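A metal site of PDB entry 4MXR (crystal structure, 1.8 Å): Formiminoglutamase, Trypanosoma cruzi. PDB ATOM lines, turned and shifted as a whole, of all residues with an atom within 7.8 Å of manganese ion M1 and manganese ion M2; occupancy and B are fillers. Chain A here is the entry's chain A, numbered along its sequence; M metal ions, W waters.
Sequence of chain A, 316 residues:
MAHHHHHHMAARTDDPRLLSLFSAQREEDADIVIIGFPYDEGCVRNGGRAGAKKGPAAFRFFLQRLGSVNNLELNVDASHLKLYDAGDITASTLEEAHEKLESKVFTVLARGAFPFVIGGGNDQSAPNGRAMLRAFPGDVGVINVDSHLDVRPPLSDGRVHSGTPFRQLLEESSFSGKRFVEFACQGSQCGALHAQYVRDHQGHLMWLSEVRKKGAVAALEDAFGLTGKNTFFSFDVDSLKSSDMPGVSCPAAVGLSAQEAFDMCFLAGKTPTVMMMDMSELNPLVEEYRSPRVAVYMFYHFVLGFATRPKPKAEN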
ATOM      1  N   ASN A  46     -15.226   7.758  10.243  1.00  0.00           N
ATOM      2  CA  ASN A  46     -14.531   9.043  10.156  1.00  0.00           C
ATOM      3  C   ASN A  46     -13.574   9.210  11.333  1.00  0.00           C
ATOM      4  O   ASN A  46     -13.008  10.283  11.539  1.00  0.00           O
ATOM      5  CB  ASN A  46     -15.551  10.187  10.126  1.00  0.00           C
ATOM      6  CG  ASN A  46     -14.956  11.499   9.636  1.00  0.00           C
ATOM      7  OD1 ASN A  46     -13.921  11.518   8.961  1.00  0.00           O
ATOM      8  ND2 ASN A  46     -15.619  12.598   9.959  1.00  0.00           N
ATOM      9  N   GLY A 121     -25.064  10.293  12.875  1.00  0.00           N
ATOM     10  CA  GLY A 121     -23.891  10.901  12.250  1.00  0.00           C
ATOM     11  C   GLY A 121     -24.212  11.786  11.059  1.00  0.00           C
ATOM     12  O   GLY A 121     -25.258  11.641  10.430  1.00  0.00           O
ATOM     13  N   ASN A 122     -23.290  12.687  10.737  1.00  0.00           N
ATOM     14  CA  ASN A 122     -23.487  13.665   9.681  1.00  0.00           C
ATOM     15  C   ASN A 122     -23.629  13.061   8.278  1.00  0.00           C
ATOM     16  O   ASN A 122     -24.023  13.752   7.335  1.00  0.00           O
ATOM     17  CB  ASN A 122     -22.352  14.699   9.690  1.00  0.00           C
ATOM     18  CG  ASN A 122     -22.840  16.111   9.399  1.00  0.00           C
ATOM     19  OD1 ASN A 122     -22.268  17.076   9.901  1.00  0.00           O
ATOM     20  ND2 ASN A 122     -23.892  16.233   8.606  1.00  0.00           N
ATOM     21  N   ASP A 123     -23.310  11.779   8.133  1.00  0.00           N
ATOM     22  CA  ASP A 123     -23.499  11.102   6.850  1.00  0.00           C
ATOM     23  C   ASP A 123     -24.961  11.149   6.403  1.00  0.00           C
ATOM     24  O   ASP A 123     -25.251  10.981   5.218  1.00  0.00           O
ATOM     25  CB  ASP A 123     -22.991   9.655   6.891  1.00  0.00           C
ATOM     26  CG  ASP A 123     -23.420   8.918   8.145  1.00  0.00           C
ATOM     27  OD1 ASP A 123     -22.891   9.223   9.238  1.00  0.00           O
ATOM     28  OD2 ASP A 123     -24.275   8.010   8.037  1.00  0.00           O
ATOM     29  N   SER A 125     -26.661  13.623   5.959  1.00  0.00           N
ATOM     30  CA  SER A 125     -26.869  14.812   5.133  1.00  0.00           C
ATOM     31  C   SER A 125     -26.756  14.540   3.638  1.00  0.00           C
ATOM     32  O   SER A 125     -27.334  15.267   2.837  1.00  0.00           O
ATOM     33  CB  SER A 125     -25.922  15.930   5.563  1.00  0.00           C
ATOM     34  OG  SER A 125     -26.099  16.214   6.936  1.00  0.00           O
ATOM     35  N   ASN A 144     -24.163  24.158   5.298  1.00  0.00           N
ATOM     36  CA  ASN A 144     -23.669  23.262   6.332  1.00  0.00           C
ATOM     37  C   ASN A 144     -23.126  24.039   7.524  1.00  0.00           C
ATOM     38  O   ASN A 144     -22.033  24.600   7.465  1.00  0.00           O
ATOM     39  CB  ASN A 144     -22.580  22.329   5.778  1.00  0.00           C
ATOM     40  CG  ASN A 144     -22.028  21.407   6.848  1.00  0.00           C
ATOM     41  OD1 ASN A 144     -22.731  21.017   7.768  1.00  0.00           O
ATOM     42  ND2 ASN A 144     -20.738  21.063   6.738  1.00  0.00           N
ATOM     43  N   VAL A 145     -23.915  24.101   8.584  1.00  0.00           N
ATOM     44  CA  VAL A 145     -23.457  24.726   9.813  1.00  0.00           C
ATOM     45  C   VAL A 145     -22.608  23.698  10.553  1.00  0.00           C
ATOM     46  O   VAL A 145     -23.132  22.681  11.044  1.00  0.00           O
ATOM     47  CB  VAL A 145     -24.626  25.185  10.701  1.00  0.00           C
ATOM     48  CG1 VAL A 145     -24.097  25.943  11.928  1.00  0.00           C
ATOM     49  CG2 VAL A 145     -25.584  26.053   9.897  1.00  0.00           C
ATOM     50  N   ASP A 146     -21.316  23.955  10.625  1.00  0.00           N
ATOM     51  CA  ASP A 146     -20.371  22.939  11.062  1.00  0.00           C
ATOM     52  C   ASP A 146     -19.004  23.587  11.291  1.00  0.00           C
ATOM     53  O   ASP A 146     -18.587  24.454  10.521  1.00  0.00           O
ATOM     54  CB  ASP A 146     -20.259  21.894   9.951  1.00  0.00           C
ATOM     55  CG  ASP A 146     -19.685  20.586  10.436  1.00  0.00           C
ATOM     56  OD1 ASP A 146     -18.931  20.582  11.428  1.00  0.00           O
ATOM     57  OD2 ASP A 146     -19.991  19.562   9.807  1.00  0.00           O
ATOM     58  N   SER A 147     -18.311  23.172  12.343  1.00  0.00           N
ATOM     59  CA  SER A 147     -16.939  23.613  12.539  1.00  0.00           C
ATOM     60  C   SER A 147     -16.023  22.973  11.499  1.00  0.00           C
ATOM     61  O   SER A 147     -14.921  23.467  11.245  1.00  0.00           O
ATOM     62  CB  SER A 147     -16.454  23.283  13.961  1.00  0.00           C
ATOM     63  OG  SER A 147     -16.601  21.905  14.232  1.00  0.00           O
ATOM     64  N   HIS A 148     -16.478  21.867  10.901  1.00  0.00           N
ATOM     65  CA  HIS A 148     -15.707  21.151   9.881  1.00  0.00           C
ATOM     66  C   HIS A 148     -16.379  21.245   8.509  1.00  0.00           C
ATOM     67  O   HIS A 148     -17.585  21.456   8.410  1.00  0.00           O
ATOM     68  CB  HIS A 148     -15.554  19.677  10.274  1.00  0.00           C
ATOM     69  CG  HIS A 148     -15.252  19.479  11.726  1.00  0.00           C
ATOM     70  ND1 HIS A 148     -16.231  19.200  12.661  1.00  0.00           N
ATOM     71  CD2 HIS A 148     -14.086  19.536  12.416  1.00  0.00           C
ATOM     72  CE1 HIS A 148     -15.680  19.084  13.860  1.00  0.00           C
ATOM     73  NE2 HIS A 148     -14.378  19.284  13.733  1.00  0.00           N
ATOM     74  N   LEU A 149     -15.586  21.086   7.449  1.00  0.00           N
ATOM     75  CA  LEU A 149     -16.117  21.211   6.084  1.00  0.00           C
ATOM     76  C   LEU A 149     -16.872  19.964   5.628  1.00  0.00           C
ATOM     77  O   LEU A 149     -17.828  20.054   4.848  1.00  0.00           O
ATOM     78  CB  LEU A 149     -14.987  21.545   5.105  1.00  0.00           C
ATOM     79  CG  LEU A 149     -14.289  22.900   5.271  1.00  0.00           C
ATOM     80  CD1 LEU A 149     -13.365  23.168   4.103  1.00  0.00           C
ATOM     81  CD2 LEU A 149     -15.322  24.003   5.410  1.00  0.00           C
ATOM     82  N   ASP A 150     -16.434  18.804   6.095  1.00  0.00           N
ATOM     83  CA  ASP A 150     -17.069  17.532   5.752  1.00  0.00           C
ATOM     84  C   ASP A 150     -17.061  17.282   4.243  1.00  0.00           C
ATOM     85  O   ASP A 150     -18.071  16.876   3.659  1.00  0.00           O
ATOM     86  CB  ASP A 150     -18.495  17.477   6.282  1.00  0.00           C
ATOM     87  CG  ASP A 150     -18.545  17.199   7.769  1.00  0.00           C
ATOM     88  OD1 ASP A 150     -17.475  17.238   8.428  1.00  0.00           O
ATOM     89  OD2 ASP A 150     -19.658  16.937   8.282  1.00  0.00           O
ATOM     90  N   SER A 162     -19.201  10.124   8.104  1.00  0.00           N
ATOM     91  CA  SER A 162     -19.714  11.388   8.604  1.00  0.00           C
ATOM     92  C   SER A 162     -18.945  12.593   8.068  1.00  0.00           C
ATOM     93  O   SER A 162     -19.384  13.734   8.223  1.00  0.00           O
ATOM     94  CB  SER A 162     -19.711  11.413  10.141  1.00  0.00           C
ATOM     95  OG  SER A 162     -18.389  11.310  10.654  1.00  0.00           O
ATOM     96  N   GLY A 163     -17.802  12.345   7.437  1.00  0.00           N
ATOM     97  CA  GLY A 163     -16.967  13.415   6.932  1.00  0.00           C
ATOM     98  C   GLY A 163     -17.036  13.673   5.436  1.00  0.00           C
ATOM     99  O   GLY A 163     -16.350  14.547   4.917  1.00  0.00           O
ATOM    100  N   THR A 164     -17.871  12.916   4.734  1.00  0.00           N
ATOM    101  CA  THR A 164     -17.944  13.027   3.276  1.00  0.00           C
ATOM    102  C   THR A 164     -19.237  13.606   2.707  1.00  0.00           C
ATOM    103  O   THR A 164     -19.333  13.780   1.488  1.00  0.00           O
ATOM    104  CB  THR A 164     -17.730  11.657   2.604  1.00  0.00           C
ATOM    105  OG1 THR A 164     -18.875  10.824   2.828  1.00  0.00           O
ATOM    106  CG2 THR A 164     -16.485  10.977   3.140  1.00  0.00           C
ATOM    107  N   PRO A 165     -20.233  13.906   3.555  1.00  0.00           N
ATOM    108  CA  PRO A 165     -21.543  14.173   2.939  1.00  0.00           C
ATOM    109  C   PRO A 165     -21.566  15.327   1.948  1.00  0.00           C
ATOM    110  O   PRO A 165     -22.292  15.260   0.963  1.00  0.00           O
ATOM    111  CB  PRO A 165     -22.439  14.494   4.147  1.00  0.00           C
ATOM    112  CG  PRO A 165     -21.494  14.991   5.181  1.00  0.00           C
ATOM    113  CD  PRO A 165     -20.263  14.142   5.005  1.00  0.00           C
ATOM    114  N   PHE A 166     -20.770  16.368   2.180  1.00  0.00           N
ATOM    115  CA  PHE A 166     -20.843  17.537   1.313  1.00  0.00           C
ATOM    116  C   PHE A 166     -19.899  17.468   0.107  1.00  0.00           C
ATOM    117  O   PHE A 166     -20.055  18.228  -0.853  1.00  0.00           O
ATOM    118  CB  PHE A 166     -20.741  18.834   2.109  1.00  0.00           C
ATOM    119  CG  PHE A 166     -21.826  18.955   3.139  1.00  0.00           C
ATOM    120  CD1 PHE A 166     -23.093  19.377   2.771  1.00  0.00           C
ATOM    121  CD2 PHE A 166     -21.608  18.577   4.452  1.00  0.00           C
ATOM    122  CE1 PHE A 166     -24.109  19.460   3.698  1.00  0.00           C
ATOM    123  CE2 PHE A 166     -22.615  18.653   5.388  1.00  0.00           C
ATOM    124  CZ  PHE A 166     -23.875  19.106   5.013  1.00  0.00           C
ATOM    125  N   GLU A 182     -20.537  26.831   3.696  1.00  0.00           N
ATOM    126  CA  GLU A 182     -19.981  26.246   4.908  1.00  0.00           C
ATOM    127  C   GLU A 182     -20.029  27.339   5.967  1.00  0.00           C
ATOM    128  O   GLU A 182     -19.315  28.346   5.857  1.00  0.00           O
ATOM    129  CB  GLU A 182     -18.535  25.806   4.673  1.00  0.00           C
ATOM    130  CG  GLU A 182     -18.352  24.706   3.630  1.00  0.00           C
ATOM    131  CD  GLU A 182     -18.575  23.305   4.173  1.00  0.00           C
ATOM    132  OE1 GLU A 182     -19.227  23.159   5.238  1.00  0.00           O
ATOM    133  OE2 GLU A 182     -18.102  22.330   3.540  1.00  0.00           O
ATOM    134  N   GLN A 189      -9.425  23.595  12.196  1.00  0.00           N
ATOM    135  CA  GLN A 189      -9.923  22.234  11.990  1.00  0.00           C
ATOM    136  C   GLN A 189     -10.164  21.920  10.514  1.00  0.00           C
ATOM    137  O   GLN A 189     -10.537  20.804  10.175  1.00  0.00           O
ATOM    138  CB  GLN A 189     -11.237  22.029  12.750  1.00  0.00           C
ATOM    139  CG  GLN A 189     -11.265  22.541  14.187  1.00  0.00           C
ATOM    140  CD  GLN A 189     -12.376  21.891  14.994  1.00  0.00           C
ATOM    141  OE1 GLN A 189     -12.370  20.672  15.208  1.00  0.00           O
ATOM    142  NE2 GLN A 189     -13.323  22.690  15.466  1.00  0.00           N
ATOM    143  N   SER A 234     -28.677  22.473   7.215  1.00  0.00           N
ATOM    144  CA  SER A 234     -28.040  21.280   7.763  1.00  0.00           C
ATOM    145  C   SER A 234     -27.126  21.648   8.937  1.00  0.00           C
ATOM    146  O   SER A 234     -26.112  22.302   8.742  1.00  0.00           O
ATOM    147  CB  SER A 234     -27.229  20.578   6.664  1.00  0.00           C
ATOM    148  OG  SER A 234     -26.692  19.335   7.101  1.00  0.00           O
ATOM    149  N   PHE A 235     -27.504  21.226  10.135  1.00  0.00           N
ATOM    150  CA  PHE A 235     -26.873  21.716  11.352  1.00  0.00           C
ATOM    151  C   PHE A 235     -26.115  20.627  12.117  1.00  0.00           C
ATOM    152  O   PHE A 235     -26.712  19.799  12.791  1.00  0.00           O
ATOM    153  CB  PHE A 235     -27.935  22.340  12.263  1.00  0.00           C
ATOM    154  CG  PHE A 235     -27.423  23.489  13.096  1.00  0.00           C
ATOM    155  CD1 PHE A 235     -26.232  23.390  13.797  1.00  0.00           C
ATOM    156  CD2 PHE A 235     -28.148  24.679  13.169  1.00  0.00           C
ATOM    157  CE1 PHE A 235     -25.781  24.449  14.573  1.00  0.00           C
ATOM    158  CE2 PHE A 235     -27.693  25.734  13.937  1.00  0.00           C
ATOM    159  CZ  PHE A 235     -26.504  25.621  14.629  1.00  0.00           C
ATOM    160  N   ASP A 236     -24.790  20.638  12.001  1.00  0.00           N
ATOM    161  CA  ASP A 236     -23.944  19.761  12.797  1.00  0.00           C
ATOM    162  C   ASP A 236     -23.718  20.433  14.143  1.00  0.00           C
ATOM    163  O   ASP A 236     -23.043  21.453  14.203  1.00  0.00           O
ATOM    164  CB  ASP A 236     -22.608  19.543  12.082  1.00  0.00           C
ATOM    165  CG  ASP A 236     -21.654  18.669  12.873  1.00  0.00           C
ATOM    166  OD1 ASP A 236     -21.793  18.553  14.104  1.00  0.00           O
ATOM    167  OD2 ASP A 236     -20.746  18.082  12.261  1.00  0.00           O
ATOM    168  N   VAL A 237     -24.286  19.870  15.203  1.00  0.00           N
ATOM    169  CA  VAL A 237     -24.237  20.538  16.509  1.00  0.00           C
ATOM    170  C   VAL A 237     -22.840  20.641  17.122  1.00  0.00           C
ATOM    171  O   VAL A 237     -22.684  21.248  18.182  1.00  0.00           O
ATOM    172  CB  VAL A 237     -25.228  19.940  17.540  1.00  0.00           C
ATOM    173  CG1 VAL A 237     -26.673  20.173  17.098  1.00  0.00           C
ATOM    174  CG2 VAL A 237     -24.949  18.456  17.756  1.00  0.00           C
ATOM    175  N   ASP A 238     -21.824  20.085  16.469  1.00  0.00           N
ATOM    176  CA  ASP A 238     -20.467  20.277  16.985  1.00  0.00           C
ATOM    177  C   ASP A 238     -19.891  21.624  16.533  1.00  0.00           C
ATOM    178  O   ASP A 238     -18.721  21.918  16.762  1.00  0.00           O
ATOM    179  CB  ASP A 238     -19.542  19.090  16.680  1.00  0.00           C
ATOM    180  CG  ASP A 238     -19.123  19.010  15.217  1.00  0.00           C
ATOM    181  OD1 ASP A 238     -19.104  20.047  14.522  1.00  0.00           O
ATOM    182  OD2 ASP A 238     -18.784  17.893  14.786  1.00  0.00           O
ATOM    183  N   SER A 239     -20.737  22.419  15.880  1.00  0.00           N
ATOM    184  CA  SER A 239     -20.398  23.807  15.557  1.00  0.00           C
ATOM    185  C   SER A 239     -20.576  24.690  16.783  1.00  0.00           C
ATOM    186  O   SER A 239     -20.093  25.827  16.811  1.00  0.00           O
ATOM    187  CB  SER A 239     -21.276  24.324  14.408  1.00  0.00           C
ATOM    188  OG  SER A 239     -22.647  24.248  14.743  1.00  0.00           O
ATOM    189  N   VAL A 248     -21.015  15.709  21.879  1.00  0.00           N
ATOM    190  CA  VAL A 248     -20.761  15.393  20.469  1.00  0.00           C
ATOM    191  C   VAL A 248     -19.451  14.621  20.367  1.00  0.00           C
ATOM    192  O   VAL A 248     -18.620  14.683  21.272  1.00  0.00           O
ATOM    193  CB  VAL A 248     -20.638  16.675  19.615  1.00  0.00           C
ATOM    194  CG1 VAL A 248     -21.951  17.412  19.552  1.00  0.00           C
ATOM    195  CG2 VAL A 248     -19.533  17.570  20.169  1.00  0.00           C
ATOM    196  N   CYS A 250     -16.924  15.186  18.360  1.00  0.00           N
ATOM    197  CA  CYS A 250     -15.807  16.114  18.244  1.00  0.00           C
ATOM    198  C   CYS A 250     -16.143  17.450  18.898  1.00  0.00           C
ATOM    199  O   CYS A 250     -16.586  18.390  18.234  1.00  0.00           O
ATOM    200  CB  CYS A 250     -15.445  16.306  16.769  1.00  0.00           C
ATOM    201  SG  CYS A 250     -13.845  17.104  16.509  1.00  0.00           S
ATOM    202  N   SER A 280     -27.113  16.838  13.100  1.00  0.00           N
ATOM    203  CA  SER A 280     -26.230  15.694  13.228  1.00  0.00           C
ATOM    204  C   SER A 280     -25.281  15.770  14.420  1.00  0.00           C
ATOM    205  O   SER A 280     -24.999  16.855  14.936  1.00  0.00           O
ATOM    206  CB  SER A 280     -25.378  15.539  11.955  1.00  0.00           C
ATOM    207  OG  SER A 280     -26.179  15.539  10.796  1.00  0.00           O
ATOM    208  N   GLU A 281     -24.795  14.606  14.844  1.00  0.00           N
ATOM    209  CA  GLU A 281     -23.670  14.464  15.768  1.00  0.00           C
ATOM    210  C   GLU A 281     -23.987  14.550  17.258  1.00  0.00           C
ATOM    211  O   GLU A 281     -23.083  14.500  18.090  1.00  0.00           O
ATOM    212  CB  GLU A 281     -22.535  15.445  15.407  1.00  0.00           C
ATOM    213  CG  GLU A 281     -21.949  15.244  13.999  1.00  0.00           C
ATOM    214  CD  GLU A 281     -21.226  13.916  13.851  1.00  0.00           C
ATOM    215  OE1 GLU A 281     -20.460  13.549  14.770  1.00  0.00           O
ATOM    216  OE2 GLU A 281     -21.410  13.249  12.806  1.00  0.00           O
HETATM  217 MN    MN M   1     -18.505  18.845  12.663  1.00  0.00          MN
HETATM  218 MN    MN M   2     -20.183  17.450  10.268  1.00  0.00          MN
HETATM  219  O   HOH W   1     -19.586  15.132  10.814  1.00  0.00           O
HETATM  220  O   HOH W   2     -18.010  17.250  10.993  1.00  0.00           O
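Water W1 lies within hydrogen-bond range of the backbone carbonyl oxygen (O) of Ser 162 (3.0 Å) and the side-chain carboxylate (OE2) of Glu 281 (3.3 Å).
Manganese ion M1 is bound by OD1 of Asp 146 (2.2 Å), OD1 of Asp 238 (2.3 Å), ND1 of His 148 (2.3 Å), OD2 of Asp 238 (2.3 Å), water W2 (2.4 Å) and OD2 of Asp 236 (2.4 Å).
Manganese ion M1 has six donor atoms within binding distance.
Manganese ion M2 is bound by OD2 of Asp 150 (2.1 Å), OD1 of Asn 122 (2.1 Å), OD2 of Asp 236 (2.2 Å), OD2 of Asp 146 (2.2 Å), water W2 (2.3 Å) and water W1 (2.5 Å).
Of the 29 residues printed, 4 come within 4 Å of manganese ion M2.
Ser 147 touches manganese ion M1 (OG to MN, 3.9 Å).
A ring nitrogen (NE2) of His 148 is in hydrogen-bond range of the side-chain amide oxygen of Gln 189, 2.9 Å away.
O of Asp 238 lies within hydrogen-bond range of OG of Ser 147 (3.3 Å).
ND2 of Asn 122 sits at hydrogen-bond distance from OG of Ser 125 (2.8 Å).
The backbone carbonyl oxygen (O) of Val 145 sits at hydrogen-bond distance from the backbone NH (N) of Asp 236.
OD2 of Asp 146 sits close to ND2 of Asn 144.
A ring nitrogen (NE2) of His 148 lies within hydrogen-bond range of the side-chain sulfur of Cys 250.
The side-chain carboxylate (OE2) of Glu 281 sits at hydrogen-bond distance from the backbone NH (N) of Asn 122 (2.9 Å).
The side-chain hydroxyl (OG) of Ser 147 lies close to a ring nitrogen (NE2) of His 148, 3.5 Å away.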
